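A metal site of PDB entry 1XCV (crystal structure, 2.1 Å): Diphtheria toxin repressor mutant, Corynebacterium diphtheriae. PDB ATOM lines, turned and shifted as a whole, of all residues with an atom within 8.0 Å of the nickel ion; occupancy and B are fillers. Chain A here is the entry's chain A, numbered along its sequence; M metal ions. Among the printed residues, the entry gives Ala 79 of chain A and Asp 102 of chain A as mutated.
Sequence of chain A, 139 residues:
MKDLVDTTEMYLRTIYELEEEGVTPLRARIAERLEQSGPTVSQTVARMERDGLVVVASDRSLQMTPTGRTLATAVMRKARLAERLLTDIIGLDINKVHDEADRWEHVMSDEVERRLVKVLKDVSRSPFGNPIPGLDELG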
ATOM      1  N   ASP A   3      17.882   0.592 -14.228  1.00  0.00           N
ATOM      2  CA  ASP A   3      16.842   1.141 -13.367  1.00  0.00           C
ATOM      3  C   ASP A   3      15.565   1.488 -14.119  1.00  0.00           C
ATOM      4  O   ASP A   3      14.479   1.472 -13.546  1.00  0.00           O
ATOM      5  CB  ASP A   3      17.382   2.352 -12.617  1.00  0.00           C
ATOM      6  CG  ASP A   3      18.386   1.957 -11.559  1.00  0.00           C
ATOM      7  OD1 ASP A   3      19.484   1.480 -11.919  1.00  0.00           O
ATOM      8  OD2 ASP A   3      18.074   2.107 -10.353  1.00  0.00           O
ATOM      9  N   LEU A   4      15.674   1.793 -15.417  1.00  0.00           N
ATOM     10  CA  LEU A   4      14.499   2.116 -16.225  1.00  0.00           C
ATOM     11  C   LEU A   4      13.879   0.826 -16.764  1.00  0.00           C
ATOM     12  O   LEU A   4      12.813   0.852 -17.375  1.00  0.00           O
ATOM     13  CB  LEU A   4      14.880   3.052 -17.396  1.00  0.00           C
ATOM     14  CG  LEU A   4      15.352   4.465 -17.018  1.00  0.00           C
ATOM     15  CD1 LEU A   4      15.656   5.257 -18.272  1.00  0.00           C
ATOM     16  CD2 LEU A   4      14.281   5.170 -16.196  1.00  0.00           C
ATOM     17  N   VAL A   5      14.559  -0.293 -16.524  1.00  0.00           N
ATOM     18  CA  VAL A   5      14.105  -1.620 -16.955  1.00  0.00           C
ATOM     19  C   VAL A   5      14.162  -1.765 -18.473  1.00  0.00           C
ATOM     20  O   VAL A   5      14.828  -2.658 -19.001  1.00  0.00           O
ATOM     21  CB  VAL A   5      12.675  -1.907 -16.445  1.00  0.00           C
ATOM     22  CG1 VAL A   5      12.277  -3.327 -16.798  1.00  0.00           C
ATOM     23  CG2 VAL A   5      12.615  -1.703 -14.925  1.00  0.00           C
ATOM     24  N   ASP A   6      13.424  -0.904 -19.184  1.00  0.00           N
ATOM     25  CA  ASP A   6      13.453  -0.906 -20.631  1.00  0.00           C
ATOM     26  C   ASP A   6      13.615   0.555 -21.030  1.00  0.00           C
ATOM     27  O   ASP A   6      12.653   1.324 -21.041  1.00  0.00           O
ATOM     28  CB  ASP A   6      12.165  -1.495 -21.236  1.00  0.00           C
ATOM     29  CG  ASP A   6      12.297  -1.734 -22.741  1.00  0.00           C
ATOM     30  OD1 ASP A   6      12.738  -0.805 -23.449  1.00  0.00           O
ATOM     31  OD2 ASP A   6      11.976  -2.852 -23.213  1.00  0.00           O
ATOM     32  N   THR A   7      14.852   0.934 -21.350  1.00  0.00           N
ATOM     33  CA  THR A   7      15.183   2.303 -21.708  1.00  0.00           C
ATOM     34  C   THR A   7      14.356   2.927 -22.825  1.00  0.00           C
ATOM     35  O   THR A   7      13.775   3.994 -22.653  1.00  0.00           O
ATOM     36  CB  THR A   7      16.670   2.407 -22.085  1.00  0.00           C
ATOM     37  OG1 THR A   7      17.464   1.997 -20.965  1.00  0.00           O
ATOM     38  CG2 THR A   7      17.028   3.844 -22.471  1.00  0.00           C
ATOM     39  N   GLU A   9      11.470   2.057 -24.126  1.00  0.00           N
ATOM     40  CA  GLU A   9      10.062   2.234 -23.769  1.00  0.00           C
ATOM     41  C   GLU A   9       9.860   3.435 -22.843  1.00  0.00           C
ATOM     42  O   GLU A   9       8.847   4.120 -22.936  1.00  0.00           O
ATOM     43  CB  GLU A   9       9.507   0.972 -23.116  1.00  0.00           C
ATOM     44  CG  GLU A   9       9.515  -0.257 -24.043  1.00  0.00           C
ATOM     45  CD  GLU A   9       8.759  -1.446 -23.468  1.00  0.00           C
ATOM     46  OE1 GLU A   9       8.546  -1.514 -22.232  1.00  0.00           O
ATOM     47  OE2 GLU A   9       8.380  -2.324 -24.268  1.00  0.00           O
ATOM     48  N   MET A  10      10.822   3.699 -21.972  1.00  0.00           N
ATOM     49  CA  MET A  10      10.705   4.849 -21.072  1.00  0.00           C
ATOM     50  C   MET A  10      10.859   6.178 -21.800  1.00  0.00           C
ATOM     51  O   MET A  10      10.267   7.183 -21.388  1.00  0.00           O
ATOM     52  CB  MET A  10      11.723   4.760 -19.933  1.00  0.00           C
ATOM     53  CG  MET A  10      11.281   3.829 -18.802  1.00  0.00           C
ATOM     54  SD  MET A  10       9.520   4.110 -18.365  1.00  0.00           S
ATOM     55  CE  MET A  10       9.640   5.485 -17.247  1.00  0.00           C
ATOM     56  N   TYR A  11      11.652   6.207 -22.878  1.00  0.00           N
ATOM     57  CA  TYR A  11      11.804   7.443 -23.646  1.00  0.00           C
ATOM     58  C   TYR A  11      10.480   7.727 -24.349  1.00  0.00           C
ATOM     59  O   TYR A  11      10.041   8.867 -24.425  1.00  0.00           O
ATOM     60  CB  TYR A  11      12.925   7.324 -24.684  1.00  0.00           C
ATOM     61  CG  TYR A  11      14.309   7.642 -24.150  1.00  0.00           C
ATOM     62  CD1 TYR A  11      14.747   7.109 -22.929  1.00  0.00           C
ATOM     63  CD2 TYR A  11      15.191   8.446 -24.858  1.00  0.00           C
ATOM     64  CE1 TYR A  11      16.029   7.362 -22.446  1.00  0.00           C
ATOM     65  CE2 TYR A  11      16.476   8.707 -24.386  1.00  0.00           C
ATOM     66  CZ  TYR A  11      16.893   8.158 -23.181  1.00  0.00           C
ATOM     67  OH  TYR A  11      18.166   8.371 -22.724  1.00  0.00           O
ATOM     68  N   ARG A  13       7.500   6.651 -23.361  1.00  0.00           N
ATOM     69  CA  ARG A  13       6.513   6.999 -22.326  1.00  0.00           C
ATOM     70  C   ARG A  13       6.688   8.463 -21.972  1.00  0.00           C
ATOM     71  O   ARG A  13       5.715   9.186 -21.759  1.00  0.00           O
ATOM     72  CB  ARG A  13       6.709   6.146 -21.060  1.00  0.00           C
ATOM     73  CG  ARG A  13       5.866   6.659 -19.877  1.00  0.00           C
ATOM     74  CD  ARG A  13       6.065   5.899 -18.571  1.00  0.00           C
ATOM     75  NE  ARG A  13       5.398   6.604 -17.469  1.00  0.00           N
ATOM     76  CZ  ARG A  13       5.149   6.079 -16.267  1.00  0.00           C
ATOM     77  NH1 ARG A  13       5.507   4.825 -16.002  1.00  0.00           N
ATOM     78  NH2 ARG A  13       4.517   6.801 -15.351  1.00  0.00           N
ATOM     79  N   LEU A  34      14.012  11.980 -16.616  1.00  0.00           N
ATOM     80  CA  LEU A  34      14.549  10.620 -16.486  1.00  0.00           C
ATOM     81  C   LEU A  34      15.937  10.698 -15.868  1.00  0.00           C
ATOM     82  O   LEU A  34      16.656   9.703 -15.789  1.00  0.00           O
ATOM     83  CB  LEU A  34      14.616   9.928 -17.851  1.00  0.00           C
ATOM     84  CG  LEU A  34      13.278   9.491 -18.445  1.00  0.00           C
ATOM     85  CD1 LEU A  34      13.519   8.750 -19.759  1.00  0.00           C
ATOM     86  CD2 LEU A  34      12.545   8.587 -17.460  1.00  0.00           C
ATOM     87  N   VAL A  75       2.616   0.968 -23.889  1.00  0.00           N
ATOM     88  CA  VAL A  75       3.342   1.050 -22.606  1.00  0.00           C
ATOM     89  C   VAL A  75       2.517   1.848 -21.601  1.00  0.00           C
ATOM     90  O   VAL A  75       2.467   1.498 -20.417  1.00  0.00           O
ATOM     91  CB  VAL A  75       4.731   1.710 -22.789  1.00  0.00           C
ATOM     92  CG1 VAL A  75       5.375   1.942 -21.428  1.00  0.00           C
ATOM     93  CG2 VAL A  75       5.628   0.796 -23.632  1.00  0.00           C
ATOM     94  N   ALA A  79       0.948   0.417 -18.112  1.00  0.00           N
ATOM     95  CA  ALA A  79       1.232   1.155 -16.879  1.00  0.00           C
ATOM     96  C   ALA A  79      -0.018   1.537 -16.115  1.00  0.00           C
ATOM     97  O   ALA A  79      -0.131   1.291 -14.911  1.00  0.00           O
ATOM     98  CB  ALA A  79       2.036   2.425 -17.187  1.00  0.00           C
ATOM     99  N   HIS A  98       2.922   4.518  -8.503  1.00  0.00           N
ATOM    100  CA  HIS A  98       3.574   5.024  -9.702  1.00  0.00           C
ATOM    101  C   HIS A  98       4.914   4.340  -9.979  1.00  0.00           C
ATOM    102  O   HIS A  98       5.174   3.935 -11.109  1.00  0.00           O
ATOM    103  CB  HIS A  98       3.757   6.546  -9.616  1.00  0.00           C
ATOM    104  CG  HIS A  98       4.621   7.114 -10.711  1.00  0.00           C
ATOM    105  ND1 HIS A  98       5.989   7.213 -10.605  1.00  0.00           N
ATOM    106  CD2 HIS A  98       4.297   7.552 -11.950  1.00  0.00           C
ATOM    107  CE1 HIS A  98       6.480   7.699 -11.740  1.00  0.00           C
ATOM    108  NE2 HIS A  98       5.475   7.913 -12.569  1.00  0.00           N
ATOM    109  N   ASP A  99       5.755   4.188  -8.970  1.00  0.00           N
ATOM    110  CA  ASP A  99       7.064   3.574  -9.179  1.00  0.00           C
ATOM    111  C   ASP A  99       6.976   2.101  -9.524  1.00  0.00           C
ATOM    112  O   ASP A  99       7.735   1.611 -10.358  1.00  0.00           O
ATOM    113  CB  ASP A  99       7.973   3.751  -7.966  1.00  0.00           C
ATOM    114  CG  ASP A  99       8.414   5.199  -7.780  1.00  0.00           C
ATOM    115  OD1 ASP A  99       8.742   5.867  -8.780  1.00  0.00           O
ATOM    116  OD2 ASP A  99       8.454   5.654  -6.615  1.00  0.00           O
ATOM    117  N   GLU A 100       6.048   1.408  -8.888  1.00  0.00           N
ATOM    118  CA  GLU A 100       5.834  -0.017  -9.110  1.00  0.00           C
ATOM    119  C   GLU A 100       5.398  -0.225 -10.562  1.00  0.00           C
ATOM    120  O   GLU A 100       6.020  -0.984 -11.308  1.00  0.00           O
ATOM    121  CB  GLU A 100       4.734  -0.542  -8.171  1.00  0.00           C
ATOM    122  CG  GLU A 100       4.622  -2.064  -8.077  1.00  0.00           C
ATOM    123  CD  GLU A 100       5.722  -2.677  -7.245  1.00  0.00           C
ATOM    124  OE1 GLU A 100       6.072  -2.077  -6.198  1.00  0.00           O
ATOM    125  OE2 GLU A 100       6.238  -3.752  -7.618  1.00  0.00           O
ATOM    126  N   ALA A 101       4.338   0.483 -10.951  1.00  0.00           N
ATOM    127  CA  ALA A 101       3.814   0.403 -12.314  1.00  0.00           C
ATOM    128  C   ALA A 101       4.870   0.805 -13.323  1.00  0.00           C
ATOM    129  O   ALA A 101       4.917   0.271 -14.427  1.00  0.00           O
ATOM    130  CB  ALA A 101       2.594   1.300 -12.461  1.00  0.00           C
ATOM    131  N   ASP A 102       5.729   1.748 -12.932  1.00  0.00           N
ATOM    132  CA  ASP A 102       6.806   2.210 -13.814  1.00  0.00           C
ATOM    133  C   ASP A 102       7.719   1.038 -14.215  1.00  0.00           C
ATOM    134  O   ASP A 102       8.349   1.072 -15.274  1.00  0.00           O
ATOM    135  CB  ASP A 102       7.623   3.292 -13.111  1.00  0.00           C
ATOM    136  CG  ASP A 102       8.396   4.176 -14.071  1.00  0.00           C
ATOM    137  OD1 ASP A 102       8.618   3.760 -15.218  1.00  0.00           O
ATOM    138  OD2 ASP A 102       8.786   5.295 -13.674  1.00  0.00           O
ATOM    139  N   ARG A 103       7.798   0.020 -13.353  1.00  0.00           N
ATOM    140  CA  ARG A 103       8.620  -1.163 -13.657  1.00  0.00           C
ATOM    141  C   ARG A 103       7.786  -2.247 -14.374  1.00  0.00           C
ATOM    142  O   ARG A 103       8.229  -2.833 -15.370  1.00  0.00           O
ATOM    143  CB  ARG A 103       9.229  -1.752 -12.374  1.00  0.00           C
ATOM    144  CG  ARG A 103      10.233  -0.838 -11.656  1.00  0.00           C
ATOM    145  CD  ARG A 103      11.101  -1.604 -10.665  1.00  0.00           C
ATOM    146  NE  ARG A 103      10.333  -2.204  -9.589  1.00  0.00           N
ATOM    147  CZ  ARG A 103       9.718  -1.511  -8.626  1.00  0.00           C
ATOM    148  NH1 ARG A 103       9.799  -0.192  -8.607  1.00  0.00           N
ATOM    149  NH2 ARG A 103       9.023  -2.143  -7.695  1.00  0.00           N
ATOM    150  N   TRP A 104       6.584  -2.492 -13.862  1.00  0.00           N
ATOM    151  CA  TRP A 104       5.669  -3.499 -14.409  1.00  0.00           C
ATOM    152  C   TRP A 104       5.266  -3.255 -15.857  1.00  0.00           C
ATOM    153  O   TRP A 104       5.077  -4.199 -16.629  1.00  0.00           O
ATOM    154  CB  TRP A 104       4.399  -3.578 -13.559  1.00  0.00           C
ATOM    155  CG  TRP A 104       4.593  -4.180 -12.191  1.00  0.00           C
ATOM    156  CD1 TRP A 104       5.720  -4.144 -11.431  1.00  0.00           C
ATOM    157  CD2 TRP A 104       3.608  -4.873 -11.417  1.00  0.00           C
ATOM    158  NE1 TRP A 104       5.502  -4.773 -10.224  1.00  0.00           N
ATOM    159  CE2 TRP A 104       4.214  -5.231 -10.189  1.00  0.00           C
ATOM    160  CE3 TRP A 104       2.264  -5.235 -11.643  1.00  0.00           C
ATOM    161  CZ2 TRP A 104       3.529  -5.929  -9.184  1.00  0.00           C
ATOM    162  CZ3 TRP A 104       1.580  -5.933 -10.639  1.00  0.00           C
ATOM    163  CH2 TRP A 104       2.222  -6.271  -9.422  1.00  0.00           C
ATOM    164  N   GLU A 105       5.105  -1.996 -16.220  1.00  0.00           N
ATOM    165  CA  GLU A 105       4.677  -1.626 -17.563  1.00  0.00           C
ATOM    166  C   GLU A 105       5.537  -2.238 -18.648  1.00  0.00           C
ATOM    167  O   GLU A 105       5.087  -2.440 -19.769  1.00  0.00           O
ATOM    168  CB  GLU A 105       4.664  -0.091 -17.700  1.00  0.00           C
ATOM    169  CG  GLU A 105       6.036   0.568 -17.778  1.00  0.00           C
ATOM    170  CD  GLU A 105       5.967   2.094 -17.749  1.00  0.00           C
ATOM    171  OE1 GLU A 105       4.975   2.658 -18.241  1.00  0.00           O
ATOM    172  OE2 GLU A 105       6.917   2.728 -17.242  1.00  0.00           O
ATOM    173  N   HIS A 106       6.783  -2.545 -18.313  1.00  0.00           N
ATOM    174  CA  HIS A 106       7.714  -3.117 -19.278  1.00  0.00           C
ATOM    175  C   HIS A 106       7.725  -4.639 -19.371  1.00  0.00           C
ATOM    176  O   HIS A 106       8.408  -5.194 -20.232  1.00  0.00           O
ATOM    177  CB  HIS A 106       9.117  -2.615 -18.959  1.00  0.00           C
ATOM    178  CG  HIS A 106       9.190  -1.125 -18.828  1.00  0.00           C
ATOM    179  ND1 HIS A 106       8.879  -0.277 -19.874  1.00  0.00           N
ATOM    180  CD2 HIS A 106       9.420  -0.334 -17.756  1.00  0.00           C
ATOM    181  CE1 HIS A 106       8.929   0.975 -19.445  1.00  0.00           C
ATOM    182  NE2 HIS A 106       9.255   0.959 -18.168  1.00  0.00           N
HETATM  183 NI    NI M   1       8.831   2.470 -16.662  1.00  0.00          NI
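OE1 of Glu 105 lies within salt-bridge range of NH1 of Arg 13 (3.2 Å). OD1 of Asp 102 lies close to NH1 of Arg 13, at 3.4 Å. ND1 of His 106 lies within hydrogen-bond range of OE1 of Glu 9, at 2.7 Å.
The nickel ion is bound by OD1 of Asp 102 (1.9 Å), OE2 of Glu 105 (2.0 Å), O of Asp 102 (2.0 Å), NE2 of His 106 (2.2 Å) and SD of Met 10 (2.5 Å). The nickel ion has five donor atoms within binding distance.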
